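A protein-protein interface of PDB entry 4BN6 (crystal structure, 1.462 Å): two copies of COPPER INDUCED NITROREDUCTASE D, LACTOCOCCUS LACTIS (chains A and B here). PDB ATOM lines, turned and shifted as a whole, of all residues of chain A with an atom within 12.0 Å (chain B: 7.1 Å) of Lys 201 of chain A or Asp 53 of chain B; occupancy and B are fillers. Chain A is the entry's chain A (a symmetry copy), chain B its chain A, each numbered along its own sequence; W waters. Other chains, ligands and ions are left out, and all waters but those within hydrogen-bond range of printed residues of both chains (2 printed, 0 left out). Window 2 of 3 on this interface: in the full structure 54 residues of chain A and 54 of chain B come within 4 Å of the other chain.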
ATOM      1  N   PHE A 197      17.772  18.235  -8.108  1.00  0.00           N
ATOM      2  CA  PHE A 197      17.891  17.797  -9.501  1.00  0.00           C
ATOM      3  C   PHE A 197      18.172  16.303  -9.581  1.00  0.00           C
ATOM      4  O   PHE A 197      19.119  15.813  -8.972  1.00  0.00           O
ATOM      5  CB  PHE A 197      19.012  18.546 -10.242  1.00  0.00           C
ATOM      6  CG  PHE A 197      18.946  20.047 -10.126  1.00  0.00           C
ATOM      7  CD1 PHE A 197      17.948  20.769 -10.754  1.00  0.00           C
ATOM      8  CD2 PHE A 197      19.923  20.741  -9.431  1.00  0.00           C
ATOM      9  CE1 PHE A 197      17.904  22.150 -10.653  1.00  0.00           C
ATOM     10  CE2 PHE A 197      19.881  22.110  -9.333  1.00  0.00           C
ATOM     11  CZ  PHE A 197      18.880  22.819  -9.949  1.00  0.00           C
ATOM     12  N   ILE A 198      17.334  15.583 -10.317  1.00  0.00           N
ATOM     13  CA  ILE A 198      17.597  14.195 -10.668  1.00  0.00           C
ATOM     14  C   ILE A 198      17.695  14.085 -12.183  1.00  0.00           C
ATOM     15  O   ILE A 198      16.817  14.550 -12.913  1.00  0.00           O
ATOM     16  CB  ILE A 198      16.486  13.249 -10.181  1.00  0.00           C
ATOM     17  CG1 ILE A 198      16.334  13.353  -8.664  1.00  0.00           C
ATOM     18  CG2 ILE A 198      16.787  11.808 -10.607  1.00  0.00           C
ATOM     19  CD1 ILE A 198      15.135  12.613  -8.114  1.00  0.00           C
ATOM     20  N   VAL A 199      18.776  13.476 -12.647  1.00  0.00           N
ATOM     21  CA  VAL A 199      18.991  13.233 -14.066  1.00  0.00           C
ATOM     22  C   VAL A 199      18.976  11.733 -14.319  1.00  0.00           C
ATOM     23  O   VAL A 199      19.688  10.975 -13.649  1.00  0.00           O
ATOM     24  CB  VAL A 199      20.339  13.830 -14.525  1.00  0.00           C
ATOM     25  CG1 VAL A 199      20.588  13.534 -15.997  1.00  0.00           C
ATOM     26  CG2 VAL A 199      20.376  15.315 -14.263  1.00  0.00           C
ATOM     27  N   ALA A 200      18.149  11.297 -15.265  1.00  0.00           N
ATOM     28  CA  ALA A 200      18.044   9.886 -15.620  1.00  0.00           C
ATOM     29  C   ALA A 200      18.066   9.720 -17.138  1.00  0.00           C
ATOM     30  O   ALA A 200      17.536  10.552 -17.873  1.00  0.00           O
ATOM     31  CB  ALA A 200      16.772   9.283 -15.039  1.00  0.00           C
ATOM     32  N   LYS A 201      18.682   8.636 -17.605  1.00  0.00           N
ATOM     33  CA  LYS A 201      18.883   8.433 -19.036  1.00  0.00           C
ATOM     34  C   LYS A 201      17.956   7.345 -19.568  1.00  0.00           C
ATOM     35  O   LYS A 201      18.403   6.267 -19.958  1.00  0.00           O
ATOM     36  CB  LYS A 201      20.331   8.076 -19.317  1.00  0.00           C
ATOM     37  N   ARG B  17      16.720  15.202 -31.876  1.00  0.00           N
ATOM     38  CA  ARG B  17      17.736  14.765 -30.925  1.00  0.00           C
ATOM     39  C   ARG B  17      19.135  15.179 -31.356  1.00  0.00           C
ATOM     40  O   ARG B  17      20.128  14.620 -30.890  1.00  0.00           O
ATOM     41  CB  ARG B  17      17.644  13.256 -30.742  1.00  0.00           C
ATOM     42  CG  ARG B  17      16.272  12.834 -30.263  1.00  0.00           C
ATOM     43  CD  ARG B  17      16.245  11.426 -29.735  1.00  0.00           C
ATOM     44  NE  ARG B  17      14.914  11.083 -29.249  1.00  0.00           N
ATOM     45  CZ  ARG B  17      14.591   9.922 -28.691  1.00  0.00           C
ATOM     46  NH1 ARG B  17      15.507   8.973 -28.533  1.00  0.00           N
ATOM     47  NH2 ARG B  17      13.348   9.713 -28.283  1.00  0.00           N
ATOM     48  N   GLU B  22      25.208  17.462 -24.265  1.00  0.00           N
ATOM     49  CA  GLU B  22      24.184  17.249 -23.248  1.00  0.00           C
ATOM     50  C   GLU B  22      24.648  17.703 -21.866  1.00  0.00           C
ATOM     51  O   GLU B  22      23.847  18.162 -21.065  1.00  0.00           O
ATOM     52  CB  GLU B  22      23.695  15.784 -23.199  1.00  0.00           C
ATOM     53  CG  GLU B  22      24.680  14.715 -23.641  1.00  0.00           C
ATOM     54  CD  GLU B  22      24.039  13.338 -23.761  1.00  0.00           C
ATOM     55  OE1 GLU B  22      23.377  12.888 -22.801  1.00  0.00           O
ATOM     56  OE2 GLU B  22      24.201  12.704 -24.826  1.00  0.00           O
ATOM     57  N   ILE B  49      15.021  15.269 -14.863  1.00  0.00           N
ATOM     58  CA  ILE B  49      15.460  15.499 -16.234  1.00  0.00           C
ATOM     59  C   ILE B  49      15.691  14.155 -16.912  1.00  0.00           C
ATOM     60  O   ILE B  49      16.565  13.388 -16.504  1.00  0.00           O
ATOM     61  CB  ILE B  49      16.761  16.328 -16.272  1.00  0.00           C
ATOM     62  CG1 ILE B  49      16.550  17.663 -15.556  1.00  0.00           C
ATOM     63  CG2 ILE B  49      17.215  16.550 -17.708  1.00  0.00           C
ATOM     64  CD1 ILE B  49      17.839  18.358 -15.156  1.00  0.00           C
ATOM     65  N   LEU B  50      14.883  13.873 -17.936  1.00  0.00           N
ATOM     66  CA  LEU B  50      14.909  12.601 -18.642  1.00  0.00           C
ATOM     67  C   LEU B  50      15.418  12.747 -20.066  1.00  0.00           C
ATOM     68  O   LEU B  50      14.953  13.607 -20.812  1.00  0.00           O
ATOM     69  CB  LEU B  50      13.504  12.000 -18.688  1.00  0.00           C
ATOM     70  CG  LEU B  50      12.806  11.830 -17.339  1.00  0.00           C
ATOM     71  CD1 LEU B  50      11.459  11.158 -17.541  1.00  0.00           C
ATOM     72  CD2 LEU B  50      13.679  11.041 -16.373  1.00  0.00           C
ATOM     73  N   THR B  51      16.372  11.901 -20.432  1.00  0.00           N
ATOM     74  CA  THR B  51      16.815  11.778 -21.820  1.00  0.00           C
ATOM     75  C   THR B  51      16.935  10.306 -22.195  1.00  0.00           C
ATOM     76  O   THR B  51      16.745   9.419 -21.360  1.00  0.00           O
ATOM     77  CB  THR B  51      18.173  12.479 -22.059  1.00  0.00           C
ATOM     78  OG1 THR B  51      19.208  11.780 -21.355  1.00  0.00           O
ATOM     79  CG2 THR B  51      18.117  13.929 -21.607  1.00  0.00           C
ATOM     80  N   GLY B  52      17.236  10.044 -23.463  1.00  0.00           N
ATOM     81  CA  GLY B  52      17.487   8.688 -23.917  1.00  0.00           C
ATOM     82  C   GLY B  52      16.378   7.707 -23.583  1.00  0.00           C
ATOM     83  O   GLY B  52      15.208   7.965 -23.848  1.00  0.00           O
ATOM     84  N   ASP B  53      16.747   6.563 -23.010  1.00  0.00           N
ATOM     85  CA  ASP B  53      15.777   5.516 -22.714  1.00  0.00           C
ATOM     86  C   ASP B  53      14.659   6.005 -21.802  1.00  0.00           C
ATOM     87  O   ASP B  53      13.522   5.554 -21.924  1.00  0.00           O
ATOM     88  CB  ASP B  53      16.456   4.312 -22.055  1.00  0.00           C
ATOM     89  CG  ASP B  53      17.303   3.512 -23.022  1.00  0.00           C
ATOM     90  OD1 ASP B  53      17.290   3.818 -24.231  1.00  0.00           O
ATOM     91  OD2 ASP B  53      17.974   2.563 -22.570  1.00  0.00           O
ATOM     92  N   ALA B  54      14.991   6.910 -20.883  1.00  0.00           N
ATOM     93  CA  ALA B  54      14.019   7.394 -19.906  1.00  0.00           C
ATOM     94  C   ALA B  54      12.999   8.297 -20.595  1.00  0.00           C
ATOM     95  O   ALA B  54      11.814   8.289 -20.248  1.00  0.00           O
ATOM     96  CB  ALA B  54      14.719   8.131 -18.771  1.00  0.00           C
ATOM     97  N   GLN B  55      13.467   9.050 -21.584  1.00  0.00           N
ATOM     98  CA  GLN B  55      12.601   9.881 -22.418  1.00  0.00           C
ATOM     99  C   GLN B  55      11.602   8.994 -23.174  1.00  0.00           C
ATOM    100  O   GLN B  55      10.402   9.268 -23.174  1.00  0.00           O
ATOM    101  CB  GLN B  55      13.456  10.720 -23.377  1.00  0.00           C
ATOM    102  CG  GLN B  55      12.737  11.297 -24.595  1.00  0.00           C
ATOM    103  CD  GLN B  55      11.762  12.400 -24.254  1.00  0.00           C
ATOM    104  OE1 GLN B  55      11.599  12.771 -23.092  1.00  0.00           O
ATOM    105  NE2 GLN B  55      11.096  12.925 -25.275  1.00  0.00           N
ATOM    106  N   ASP B  56      12.088   7.921 -23.797  1.00  0.00           N
ATOM    107  CA  ASP B  56      11.200   6.976 -24.484  1.00  0.00           C
ATOM    108  C   ASP B  56      10.171   6.380 -23.525  1.00  0.00           C
ATOM    109  O   ASP B  56       8.993   6.247 -23.857  1.00  0.00           O
ATOM    110  CB  ASP B  56      11.999   5.836 -25.114  1.00  0.00           C
ATOM    111  CG  ASP B  56      12.828   6.279 -26.296  1.00  0.00           C
ATOM    112  OD1 ASP B  56      12.628   7.408 -26.781  1.00  0.00           O
ATOM    113  OD2 ASP B  56      13.670   5.477 -26.757  1.00  0.00           O
ATOM    114  N   LYS B  57      10.627   6.012 -22.335  1.00  0.00           N
ATOM    115  CA  LYS B  57       9.771   5.333 -21.375  1.00  0.00           C
ATOM    116  C   LYS B  57       8.643   6.235 -20.891  1.00  0.00           C
ATOM    117  O   LYS B  57       7.500   5.799 -20.778  1.00  0.00           O
ATOM    118  CB  LYS B  57      10.591   4.840 -20.184  1.00  0.00           C
ATOM    119  CG  LYS B  57       9.755   4.150 -19.118  1.00  0.00           C
ATOM    120  CD  LYS B  57      10.620   3.479 -18.070  1.00  0.00           C
ATOM    121  CE  LYS B  57      11.312   2.246 -18.626  1.00  0.00           C
ATOM    122  NZ  LYS B  57      11.979   1.453 -17.558  1.00  0.00           N
ATOM    123  N   LEU B  58       8.962   7.489 -20.597  1.00  0.00           N
ATOM    124  CA  LEU B  58       7.949   8.411 -20.110  1.00  0.00           C
ATOM    125  C   LEU B  58       6.772   8.450 -21.079  1.00  0.00           C
ATOM    126  O   LEU B  58       5.626   8.274 -20.680  1.00  0.00           O
ATOM    127  CB  LEU B  58       8.528   9.816 -19.931  1.00  0.00           C
ATOM    128  CG  LEU B  58       7.499  10.895 -19.581  1.00  0.00           C
ATOM    129  CD1 LEU B  58       6.859  10.614 -18.232  1.00  0.00           C
ATOM    130  CD2 LEU B  58       8.124  12.288 -19.610  1.00  0.00           C
ATOM    131  N   GLU B  61       5.448   4.431 -22.172  1.00  0.00           N
ATOM    132  CA  GLU B  61       4.994   3.523 -21.124  1.00  0.00           C
ATOM    133  C   GLU B  61       4.163   4.193 -20.033  1.00  0.00           C
ATOM    134  O   GLU B  61       3.481   3.509 -19.267  1.00  0.00           O
ATOM    135  CB  GLU B  61       6.189   2.802 -20.496  1.00  0.00           C
ATOM    136  CG  GLU B  61       6.952   1.927 -21.476  1.00  0.00           C
ATOM    137  CD  GLU B  61       7.971   1.038 -20.795  1.00  0.00           C
ATOM    138  OE1 GLU B  61       7.639   0.441 -19.749  1.00  0.00           O
ATOM    139  OE2 GLU B  61       9.104   0.937 -21.307  1.00  0.00           O
ATOM    140  N   TRP B 164      10.677   6.613 -11.067  1.00  0.00           N
ATOM    141  CA  TRP B 164      11.932   7.285 -10.737  1.00  0.00           C
ATOM    142  C   TRP B 164      12.078   7.534  -9.229  1.00  0.00           C
ATOM    143  O   TRP B 164      12.892   8.357  -8.794  1.00  0.00           O
ATOM    144  CB  TRP B 164      12.091   8.567 -11.576  1.00  0.00           C
ATOM    145  CG  TRP B 164      12.363   8.225 -13.023  1.00  0.00           C
ATOM    146  CD1 TRP B 164      13.555   7.829 -13.553  1.00  0.00           C
ATOM    147  CD2 TRP B 164      11.418   8.204 -14.102  1.00  0.00           C
ATOM    148  NE1 TRP B 164      13.416   7.564 -14.893  1.00  0.00           N
ATOM    149  CE2 TRP B 164      12.113   7.782 -15.256  1.00  0.00           C
ATOM    150  CE3 TRP B 164      10.053   8.495 -14.208  1.00  0.00           C
ATOM    151  CZ2 TRP B 164      11.491   7.651 -16.498  1.00  0.00           C
ATOM    152  CZ3 TRP B 164       9.437   8.362 -15.446  1.00  0.00           C
ATOM    153  CH2 TRP B 164      10.156   7.946 -16.572  1.00  0.00           C
HETATM  154  O   HOH W   1      19.495  12.534 -18.806  1.00  0.00           O
HETATM  155  O   HOH W   2      19.501   5.929 -22.567  1.00  0.00           O
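No position is printed for both chains.
Among the printed residues, merely in contact across the chains: Lys 201 of chain A with Thr 51 of chain B, Lys 201 of chain A with Ala 54 of chain B, Ala 200 of chain A with Leu 50 of chain B, Val 199 of chain A with Ile 49 of chain B, Ala 200 of chain A with Trp 164 of chain B and Ala 200 of chain A with Ala 54 of chain B.
Hydrophobic or aromatic side chains of chain B within 4 Å of the printed part of chain A: Ile 49, Leu 50, Ala 54 and Trp 164. Of the 5 printed residues of chain A, 4 touch a printed residue of chain B.
Water W1 lies within hydrogen-bond range of the side-chain hydroxyl (OG1) of Thr 51 of chain B (2.7 Å) and the backbone carbonyl oxygen (O) of Ala 200 of chain A (2.9 Å). Water W2 bridges the backbone carbonyl oxygen (O) of Lys 201 of chain A (2.9 Å) and the backbone NH (N) of Asp 53 of chain B (2.9 Å).
Lys 201 of chain A touches three residues of chain B. Of chain A, only Lys 201 (3.5 Å) comes within 4 Å of Asp 53 of chain B. Of the printed residues of chain A, Thr 51 of chain B touches Ala 200 (3.1 Å) and Lys 201 (3.0 Å). No residue of chain A comes within 4 Å of Gly 52 of chain B. Of chain A, only Ala 200 (3.8 Å) and Lys 201 (3.3 Å) come within 4 Å of Ala 54 of chain B. Of the printed residues of chain B, Ile 198 of chain A touches Ile 49. Of the printed residues of chain A, Trp 164 of chain B touches Ala 200 (3.8 Å). Printed residues of chain A within 4 Å of Ile 49 of chain B: Ile 198 (2.7 Å), Val 199 (3.4 Å) and Ala 200 (2.9 Å). Of the printed residues of chain B, Ala 200 of chain A touches Ile 49 (2.9 Å), Leu 50 (3.4 Å), Thr 51 (3.1 Å), Ala 54 (3.8 Å) and Trp 164 (3.8 Å). Of the printed residues of chain B, Val 199 of chain A touches Ile 49. The nearest residue of chain B that does not touch Lys 201 of chain A is Gly 52 of chain B (4.3 Å). The nearest residue of chain A that does not touch Asp 53 of chain B is Ala 200 of chain A (6.6 Å). The nearest printed residue of chain A that does not touch Ile 49 of chain B is Phe 197 of chain A (5.0 Å).
The backbone NH (N) of Ile 49 of chain B is in hydrogen-bond range of the backbone carbonyl oxygen (O) of Ile 198 of chain A (2.7 Å). The backbone NH (N) of Ala 200 of chain A is in hydrogen-bond range of the backbone carbonyl oxygen (O) of Ile 49 of chain B. The backbone carbonyl oxygen of Ala 200 of chain A sits at hydrogen-bond distance from the backbone NH of Thr 51 of chain B (3.1 Å). O of Lys 201 of chain A lies close to N of Asp 53 of chain B.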
